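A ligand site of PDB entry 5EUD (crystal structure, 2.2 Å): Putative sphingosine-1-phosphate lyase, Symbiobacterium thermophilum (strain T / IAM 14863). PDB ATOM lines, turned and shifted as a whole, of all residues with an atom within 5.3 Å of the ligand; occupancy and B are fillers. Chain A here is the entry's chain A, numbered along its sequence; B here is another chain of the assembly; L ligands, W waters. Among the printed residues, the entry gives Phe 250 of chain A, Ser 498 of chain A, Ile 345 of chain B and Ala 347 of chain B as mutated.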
ATOM      1  N   HIS A 202      16.137  21.749  18.151  1.00  0.00           N
ATOM      2  CA  HIS A 202      15.066  22.091  17.217  1.00  0.00           C
ATOM      3  C   HIS A 202      14.183  23.233  17.682  1.00  0.00           C
ATOM      4  O   HIS A 202      13.816  23.301  18.863  1.00  0.00           O
ATOM      5  CB  HIS A 202      14.241  20.844  16.877  1.00  0.00           C
ATOM      6  CG  HIS A 202      13.457  20.988  15.606  1.00  0.00           C
ATOM      7  ND1 HIS A 202      12.261  21.671  15.559  1.00  0.00           N
ATOM      8  CD2 HIS A 202      13.784  20.618  14.341  1.00  0.00           C
ATOM      9  CE1 HIS A 202      11.861  21.655  14.311  1.00  0.00           C
ATOM     10  NE2 HIS A 202      12.731  21.023  13.530  1.00  0.00           N
ATOM     11  N   PHE A 250      19.843  19.426  14.047  1.00  0.00           N
ATOM     12  CA  PHE A 250      19.691  19.814  12.641  1.00  0.00           C
ATOM     13  C   PHE A 250      20.759  20.814  12.181  1.00  0.00           C
ATOM     14  O   PHE A 250      21.218  20.634  11.065  1.00  0.00           O
ATOM     15  CB  PHE A 250      18.291  20.421  12.365  1.00  0.00           C
ATOM     16  CG  PHE A 250      18.064  21.057  10.994  1.00  0.00           C
ATOM     17  CD1 PHE A 250      17.672  20.273   9.902  1.00  0.00           C
ATOM     18  CD2 PHE A 250      18.203  22.431  10.812  1.00  0.00           C
ATOM     19  CE1 PHE A 250      17.416  20.868   8.656  1.00  0.00           C
ATOM     20  CE2 PHE A 250      17.947  23.014   9.558  1.00  0.00           C
ATOM     21  CZ  PHE A 250      17.532  22.234   8.510  1.00  0.00           C
ATOM     22  N1  LLP A 312      14.048  17.537  15.081  1.00  0.00           N
ATOM     23  C2  LLP A 312      15.064  17.346  14.200  1.00  0.00           C
ATOM     24  C2' LLP A 312      16.456  17.365  14.799  1.00  0.00           C
ATOM     25  C3  LLP A 312      14.771  17.169  12.786  1.00  0.00           C
ATOM     26  O3  LLP A 312      15.765  16.970  11.905  1.00  0.00           O
ATOM     27  C4  LLP A 312      13.415  17.144  12.347  1.00  0.00           C
ATOM     28  C4' LLP A 312      12.949  16.943  10.854  1.00  0.00           C
ATOM     29  C5  LLP A 312      12.420  17.404  13.367  1.00  0.00           C
ATOM     30  C6  LLP A 312      12.739  17.582  14.716  1.00  0.00           C
ATOM     31  C5' LLP A 312      10.978  17.496  13.109  1.00  0.00           C
ATOM     32  OP4 LLP A 312      10.656  18.320  12.017  1.00  0.00           O
ATOM     33  P   LLP A 312       9.479  17.750  11.250  1.00  0.00           P
ATOM     34  OP1 LLP A 312       9.423  16.293  10.884  1.00  0.00           O
ATOM     35  OP2 LLP A 312       8.176  18.033  12.030  1.00  0.00           O
ATOM     36  OP3 LLP A 312       9.480  18.650  10.047  1.00  0.00           O
ATOM     37  N   LLP A 312      11.692  10.472   7.741  1.00  0.00           N
ATOM     38  CA  LLP A 312      13.025  10.931   7.378  1.00  0.00           C
ATOM     39  CB  LLP A 312      13.774  11.778   8.404  1.00  0.00           C
ATOM     40  CG  LLP A 312      13.245  13.177   8.385  1.00  0.00           C
ATOM     41  CD  LLP A 312      14.053  13.942   9.418  1.00  0.00           C
ATOM     42  CE  LLP A 312      13.014  14.902   9.976  1.00  0.00           C
ATOM     43  NZ  LLP A 312      13.660  16.147   9.898  1.00  0.00           N
ATOM     44  C   LLP A 312      13.769   9.699   6.831  1.00  0.00           C
ATOM     45  O   LLP A 312      13.332   9.127   5.816  1.00  0.00           O
ATOM     46  N   ASN A 433      20.188  24.497   2.903  1.00  0.00           N
ATOM     47  CA  ASN A 433      19.600  25.141   4.074  1.00  0.00           C
ATOM     48  C   ASN A 433      20.522  26.273   4.573  1.00  0.00           C
ATOM     49  O   ASN A 433      21.712  26.040   4.824  1.00  0.00           O
ATOM     50  CB  ASN A 433      19.348  24.099   5.172  1.00  0.00           C
ATOM     51  CG  ASN A 433      18.449  22.959   4.736  1.00  0.00           C
ATOM     52  OD1 ASN A 433      18.892  21.920   4.269  1.00  0.00           O
ATOM     53  ND2 ASN A 433      17.171  23.082   4.904  1.00  0.00           N
ATOM     54  N   VAL A 482      19.364  39.179   1.791  1.00  0.00           N
ATOM     55  CA  VAL A 482      18.199  38.832   2.623  1.00  0.00           C
ATOM     56  C   VAL A 482      18.690  38.062   3.838  1.00  0.00           C
ATOM     57  O   VAL A 482      18.326  38.396   4.965  1.00  0.00           O
ATOM     58  CB  VAL A 482      17.108  38.044   1.863  1.00  0.00           C
ATOM     59  CG1 VAL A 482      15.753  38.170   2.573  1.00  0.00           C
ATOM     60  CG2 VAL A 482      16.996  38.475   0.406  1.00  0.00           C
ATOM     61  N   TYR A 483      19.543  37.044   3.608  1.00  0.00           N
ATOM     62  CA  TYR A 483      20.159  36.207   4.644  1.00  0.00           C
ATOM     63  C   TYR A 483      21.077  37.044   5.532  1.00  0.00           C
ATOM     64  O   TYR A 483      21.060  36.874   6.752  1.00  0.00           O
ATOM     65  CB  TYR A 483      20.906  35.031   4.000  1.00  0.00           C
ATOM     66  CG  TYR A 483      20.015  33.859   3.651  1.00  0.00           C
ATOM     67  CD1 TYR A 483      19.365  33.795   2.422  1.00  0.00           C
ATOM     68  CD2 TYR A 483      19.807  32.817   4.545  1.00  0.00           C
ATOM     69  CE1 TYR A 483      18.526  32.721   2.103  1.00  0.00           C
ATOM     70  CE2 TYR A 483      18.977  31.744   4.238  1.00  0.00           C
ATOM     71  CZ  TYR A 483      18.346  31.694   3.002  1.00  0.00           C
ATOM     72  OH  TYR A 483      17.533  30.640   2.679  1.00  0.00           O
ATOM     73  N   ALA A 486      18.772  39.273   7.609  1.00  0.00           N
ATOM     74  CA  ALA A 486      18.138  38.360   8.577  1.00  0.00           C
ATOM     75  C   ALA A 486      19.018  38.010   9.776  1.00  0.00           C
ATOM     76  O   ALA A 486      18.548  38.038  10.914  1.00  0.00           O
ATOM     77  CB  ALA A 486      17.686  37.101   7.862  1.00  0.00           C
ATOM     78  N   VAL A 497       8.905  40.228   8.766  1.00  0.00           N
ATOM     79  CA  VAL A 497       9.251  39.702   7.430  1.00  0.00           C
ATOM     80  C   VAL A 497       8.732  38.244   7.242  1.00  0.00           C
ATOM     81  O   VAL A 497       8.227  37.913   6.158  1.00  0.00           O
ATOM     82  CB  VAL A 497      10.776  39.885   7.124  1.00  0.00           C
ATOM     83  CG1 VAL A 497      11.123  39.404   5.720  1.00  0.00           C
ATOM     84  CG2 VAL A 497      11.172  41.347   7.254  1.00  0.00           C
ATOM     85  N   SER A 498       8.813  37.413   8.304  1.00  0.00           N
ATOM     86  CA  SER A 498       8.357  36.006   8.295  1.00  0.00           C
ATOM     87  C   SER A 498       6.827  35.912   8.150  1.00  0.00           C
ATOM     88  O   SER A 498       6.329  35.084   7.403  1.00  0.00           O
ATOM     89  CB  SER A 498       8.834  35.281   9.545  1.00  0.00           C
ATOM     90  OG  SER A 498      10.248  35.186   9.539  1.00  0.00           O
ATOM     91  N   PHE A 501       6.012  36.699   4.595  1.00  0.00           N
ATOM     92  CA  PHE A 501       6.390  35.593   3.718  1.00  0.00           C
ATOM     93  C   PHE A 501       5.309  34.514   3.713  1.00  0.00           C
ATOM     94  O   PHE A 501       4.974  33.996   2.642  1.00  0.00           O
ATOM     95  CB  PHE A 501       7.767  35.021   4.108  1.00  0.00           C
ATOM     96  CG  PHE A 501       8.142  33.716   3.440  1.00  0.00           C
ATOM     97  CD1 PHE A 501       8.558  33.679   2.112  1.00  0.00           C
ATOM     98  CD2 PHE A 501       8.116  32.520   4.146  1.00  0.00           C
ATOM     99  CE1 PHE A 501       8.926  32.473   1.512  1.00  0.00           C
ATOM    100  CE2 PHE A 501       8.491  31.309   3.541  1.00  0.00           C
ATOM    101  CZ  PHE A 501       8.877  31.299   2.224  1.00  0.00           C
ATOM    102  N   LEU A 505       2.602  33.189   0.687  1.00  0.00           N
ATOM    103  CA  LEU A 505       2.323  31.803   0.316  1.00  0.00           C
ATOM    104  C   LEU A 505       0.834  31.532   0.092  1.00  0.00           C
ATOM    105  O   LEU A 505       0.490  30.791  -0.835  1.00  0.00           O
ATOM    106  CB  LEU A 505       2.916  30.813   1.339  1.00  0.00           C
ATOM    107  CG  LEU A 505       4.425  30.692   1.334  1.00  0.00           C
ATOM    108  CD1 LEU A 505       4.895  29.808   2.478  1.00  0.00           C
ATOM    109  CD2 LEU A 505       4.933  30.154   0.018  1.00  0.00           C
ATOM    110  N   PRO B 128       5.116  20.843   2.193  1.00  0.00           N
ATOM    111  CA  PRO B 128       4.911  22.313   2.132  1.00  0.00           C
ATOM    112  C   PRO B 128       5.816  23.167   3.046  1.00  0.00           C
ATOM    113  O   PRO B 128       5.769  24.385   2.967  1.00  0.00           O
ATOM    114  CB  PRO B 128       3.419  22.504   2.413  1.00  0.00           C
ATOM    115  CG  PRO B 128       2.972  21.243   3.037  1.00  0.00           C
ATOM    116  CD  PRO B 128       3.872  20.144   2.572  1.00  0.00           C
ATOM    117  N   LEU B 129       6.646  22.532   3.845  1.00  0.00           N
ATOM    118  CA  LEU B 129       7.695  23.205   4.584  1.00  0.00           C
ATOM    119  C   LEU B 129       8.724  23.815   3.627  1.00  0.00           C
ATOM    120  O   LEU B 129       9.357  24.764   3.927  1.00  0.00           O
ATOM    121  CB  LEU B 129       8.343  22.230   5.547  1.00  0.00           C
ATOM    122  CG  LEU B 129       9.490  22.592   6.473  1.00  0.00           C
ATOM    123  CD1 LEU B 129       9.084  23.639   7.475  1.00  0.00           C
ATOM    124  CD2 LEU B 129      10.066  21.373   7.164  1.00  0.00           C
ATOM    125  N   HIS B 130       8.823  23.239   2.441  1.00  0.00           N
ATOM    126  CA  HIS B 130       9.695  23.674   1.362  1.00  0.00           C
ATOM    127  C   HIS B 130       8.849  24.213   0.172  1.00  0.00           C
ATOM    128  O   HIS B 130       8.667  23.492  -0.810  1.00  0.00           O
ATOM    129  CB  HIS B 130      10.602  22.518   0.906  1.00  0.00           C
ATOM    130  CG  HIS B 130      11.303  21.848   2.049  1.00  0.00           C
ATOM    131  ND1 HIS B 130      12.554  22.256   2.461  1.00  0.00           N
ATOM    132  CD2 HIS B 130      10.876  20.841   2.839  1.00  0.00           C
ATOM    133  CE1 HIS B 130      12.855  21.481   3.492  1.00  0.00           C
ATOM    134  NE2 HIS B 130      11.878  20.631   3.779  1.00  0.00           N
ATOM    135  N   PRO B 131       8.319  25.475   0.257  1.00  0.00           N
ATOM    136  CA  PRO B 131       7.544  26.010  -0.889  1.00  0.00           C
ATOM    137  C   PRO B 131       8.399  26.319  -2.122  1.00  0.00           C
ATOM    138  O   PRO B 131       7.863  26.431  -3.232  1.00  0.00           O
ATOM    139  CB  PRO B 131       6.868  27.261  -0.306  1.00  0.00           C
ATOM    140  CG  PRO B 131       7.746  27.704   0.802  1.00  0.00           C
ATOM    141  CD  PRO B 131       8.419  26.462   1.349  1.00  0.00           C
ATOM    142  N   TRP B 341      17.350  30.705  16.446  1.00  0.00           N
ATOM    143  CA  TRP B 341      17.794  29.313  16.316  1.00  0.00           C
ATOM    144  C   TRP B 341      18.920  29.177  15.291  1.00  0.00           C
ATOM    145  O   TRP B 341      18.697  29.545  14.131  1.00  0.00           O
ATOM    146  CB  TRP B 341      16.612  28.413  15.915  1.00  0.00           C
ATOM    147  CG  TRP B 341      16.932  26.956  15.779  1.00  0.00           C
ATOM    148  CD1 TRP B 341      17.628  26.170  16.650  1.00  0.00           C
ATOM    149  CD2 TRP B 341      16.450  26.084  14.755  1.00  0.00           C
ATOM    150  NE1 TRP B 341      17.692  24.880  16.176  1.00  0.00           N
ATOM    151  CE2 TRP B 341      16.948  24.785  15.030  1.00  0.00           C
ATOM    152  CE3 TRP B 341      15.690  26.277  13.585  1.00  0.00           C
ATOM    153  CZ2 TRP B 341      16.660  23.686  14.218  1.00  0.00           C
ATOM    154  CZ3 TRP B 341      15.391  25.183  12.791  1.00  0.00           C
ATOM    155  CH2 TRP B 341      15.895  23.915  13.086  1.00  0.00           C
ATOM    156  N   GLY B 343      19.576  26.895  13.389  1.00  0.00           N
ATOM    157  CA  GLY B 343      19.048  26.178  12.234  1.00  0.00           C
ATOM    158  C   GLY B 343      18.438  27.067  11.171  1.00  0.00           C
ATOM    159  O   GLY B 343      17.930  26.569  10.159  1.00  0.00           O
ATOM    160  N   GLY B 344      18.489  28.376  11.402  1.00  0.00           N
ATOM    161  CA  GLY B 344      17.960  29.398  10.496  1.00  0.00           C
ATOM    162  C   GLY B 344      16.645  29.981  10.980  1.00  0.00           C
ATOM    163  O   GLY B 344      16.096  29.524  11.992  1.00  0.00           O
ATOM    164  N   ILE B 345      16.140  31.003  10.253  1.00  0.00           N
ATOM    165  CA  ILE B 345      14.836  31.624  10.528  1.00  0.00           C
ATOM    166  C   ILE B 345      13.783  30.571  10.229  1.00  0.00           C
ATOM    167  O   ILE B 345      13.789  29.948   9.165  1.00  0.00           O
ATOM    168  CB  ILE B 345      14.624  32.983   9.820  1.00  0.00           C
ATOM    169  CG1 ILE B 345      15.501  34.056  10.521  1.00  0.00           C
ATOM    170  CG2 ILE B 345      13.154  33.398   9.893  1.00  0.00           C
ATOM    171  CD1 ILE B 345      15.639  35.303   9.778  1.00  0.00           C
ATOM    172  N   TYR B 346      12.950  30.300  11.228  1.00  0.00           N
ATOM    173  CA  TYR B 346      11.952  29.256  11.182  1.00  0.00           C
ATOM    174  C   TYR B 346      10.571  29.841  11.448  1.00  0.00           C
ATOM    175  O   TYR B 346      10.329  30.435  12.491  1.00  0.00           O
ATOM    176  CB  TYR B 346      12.341  28.171  12.219  1.00  0.00           C
ATOM    177  CG  TYR B 346      11.559  26.897  12.073  1.00  0.00           C
ATOM    178  CD1 TYR B 346      10.331  26.732  12.722  1.00  0.00           C
ATOM    179  CD2 TYR B 346      12.026  25.849  11.302  1.00  0.00           C
ATOM    180  CE1 TYR B 346       9.590  25.567  12.579  1.00  0.00           C
ATOM    181  CE2 TYR B 346      11.292  24.666  11.146  1.00  0.00           C
ATOM    182  CZ  TYR B 346      10.091  24.527  11.807  1.00  0.00           C
ATOM    183  OH  TYR B 346       9.365  23.369  11.678  1.00  0.00           O
ATOM    184  N   ALA B 347       9.685  29.696  10.479  1.00  0.00           N
ATOM    185  CA  ALA B 347       8.309  30.167  10.546  1.00  0.00           C
ATOM    186  C   ALA B 347       7.334  28.993  10.262  1.00  0.00           C
ATOM    187  O   ALA B 347       7.557  28.231   9.329  1.00  0.00           O
ATOM    188  CB  ALA B 347       8.096  31.287   9.558  1.00  0.00           C
ATOM    189  N   SER B 348       6.321  28.836  11.129  1.00  0.00           N
ATOM    190  CA  SER B 348       5.295  27.805  10.987  1.00  0.00           C
ATOM    191  C   SER B 348       3.909  28.435  10.931  1.00  0.00           C
ATOM    192  O   SER B 348       3.510  29.071  11.912  1.00  0.00           O
ATOM    193  CB  SER B 348       5.321  26.838  12.177  1.00  0.00           C
ATOM    194  OG  SER B 348       6.323  25.854  12.061  1.00  0.00           O
ATOM    195  N   PRO B 349       3.120  28.234   9.856  1.00  0.00           N
ATOM    196  CA  PRO B 349       1.749  28.791   9.858  1.00  0.00           C
ATOM    197  C   PRO B 349       0.803  28.015  10.785  1.00  0.00           C
ATOM    198  O   PRO B 349      -0.188  28.577  11.263  1.00  0.00           O
ATOM    199  CB  PRO B 349       1.318  28.721   8.397  1.00  0.00           C
ATOM    200  CG  PRO B 349       2.143  27.624   7.802  1.00  0.00           C
ATOM    201  CD  PRO B 349       3.418  27.508   8.603  1.00  0.00           C
HETATM  202  C1  LIG L   1      14.268  22.687   9.639  1.00  0.00           C
HETATM  203  C2  LIG L   1      14.378  21.623  10.174  1.00  0.00           C
HETATM  204  C3  LIG L   1      14.819  25.025   9.263  1.00  0.00           C
HETATM  205  C4  LIG L   1      13.023  23.970   8.088  1.00  0.00           C
HETATM  206  C5  LIG L   1      14.539  26.216   8.615  1.00  0.00           C
HETATM  207  C6  LIG L   1      12.758  25.156   7.447  1.00  0.00           C
HETATM  208  C7  LIG L   1      14.695  32.537   5.287  1.00  0.00           C
HETATM  209  C8  LIG L   1      12.473  33.599   6.541  1.00  0.00           C
HETATM  210  C9  LIG L   1       8.267  27.484   6.418  1.00  0.00           C
HETATM  211  C10 LIG L   1      14.048  23.918   8.994  1.00  0.00           C
HETATM  212  C11 LIG L   1      13.512  26.284   7.709  1.00  0.00           C
HETATM  213  C12 LIG L   1      13.598  31.728   5.564  1.00  0.00           C
HETATM  214  C13 LIG L   1      14.688  33.872   5.633  1.00  0.00           C
HETATM  215  C14 LIG L   1      12.471  32.263   6.185  1.00  0.00           C
HETATM  216  C15 LIG L   1      13.563  34.401   6.262  1.00  0.00           C
HETATM  217  C16 LIG L   1       9.599  27.840   6.083  1.00  0.00           C
HETATM  218  C17 LIG L   1       7.592  27.506   5.227  1.00  0.00           C
HETATM  219  C18 LIG L   1      10.720  27.960   6.963  1.00  0.00           C
HETATM  220  C19 LIG L   1      15.892  34.685   5.300  1.00  0.00           C
HETATM  221  C20 LIG L   1      11.264  31.473   6.509  1.00  0.00           C
HETATM  222  C21 LIG L   1       6.207  27.236   4.824  1.00  0.00           C
HETATM  223  C22 LIG L   1      12.598  36.352   5.748  1.00  0.00           C
HETATM  224  C23 LIG L   1      14.452  20.320  10.811  1.00  0.00           C
HETATM  225  C24 LIG L   1      13.683  30.307   5.157  1.00  0.00           C
HETATM  226  C25 LIG L   1      14.240  28.081   6.057  1.00  0.00           C
HETATM  227  C26 LIG L   1      13.171  27.578   7.008  1.00  0.00           C
HETATM  228  N1  LIG L   1       9.729  28.053   4.773  1.00  0.00           N
HETATM  229  N2  LIG L   1      11.885  27.550   6.345  1.00  0.00           N
HETATM  230  N3  LIG L   1      14.296  29.535   6.262  1.00  0.00           N
HETATM  231  O1  LIG L   1      10.610  28.365   8.110  1.00  0.00           O
HETATM  232  O2  LIG L   1       8.469  27.851   4.232  1.00  0.00           O
HETATM  233  O3  LIG L   1      13.124  19.905  11.032  1.00  0.00           O
HETATM  234  O4  LIG L   1      13.512  35.732   6.650  1.00  0.00           O
HETATM  235  O   HOH W   1      10.764  21.179  11.066  1.00  0.00           O
HETATM  236  O   HOH W   2      16.223  25.569   5.355  1.00  0.00           O
HETATM  237  O   HOH W   3      17.665  26.738   7.312  1.00  0.00           O
HETATM  238  O   HOH W   4      11.895  28.105   2.213  1.00  0.00           O
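Water W1 lies within hydrogen-bond range of OH of Tyr 346 of chain B (2.7 Å), O3 of the ligand (2.7 Å), OP3 of LLP 312 (3.0 Å) and NE2 of His 202 (3.2 Å).
NE2 of His 202 is in hydrogen-bond range of O3 of the ligand (2.8 Å).
O1 of the ligand is in hydrogen-bond range of N of Ala 347 of chain B (2.9 Å).
An oxygen (O3) of the ligand sits close to OP4 of LLP 312, at 3.1 Å.
The backbone carbonyl oxygen of Ile 345 of chain B lies within hydrogen-bond range of a nitrogen (N3) of the ligand.
O of Leu 129 of chain B sits close to O2 of the ligand (3.2 Å).
Phe 250 touches the ligand (CD1 to C23, 3.3 Å).
CB of Ala 486 touches C19 of the ligand (3.95 Å).
CG1 of Val 497 touches C22 of the ligand, at 3.4 Å.
CE2 of Phe 501 touches O2 of the ligand, 3.5 Å away.
CD1 of Leu 505 touches C21 of the ligand, at 3.7 Å.
Pro 128 of chain B touches the ligand.
Pro 131 of chain B touches the ligand (CD to O2, 3.2 Å).
Trp 341 of chain B touches the ligand.
Gly 343 of chain B touches the ligand.
CA of Tyr 346 of chain B touches O1 of the ligand, 3.5 Å away.
Hydrophobic or aromatic side chains within 4 Å of the ligand: His 202, Phe 250, Ala 486, Val 497, Phe 501, Leu 505, Leu 129 of chain B, Pro 131 of chain B, Trp 341 of chain B, Ile 345 of chain B and Tyr 346 of chain B.
Of the 23 residues printed, 15 come within 4 Å of the ligand.
The nearest printed residue that does not touch the ligand is Ser 498 (4.1 Å).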
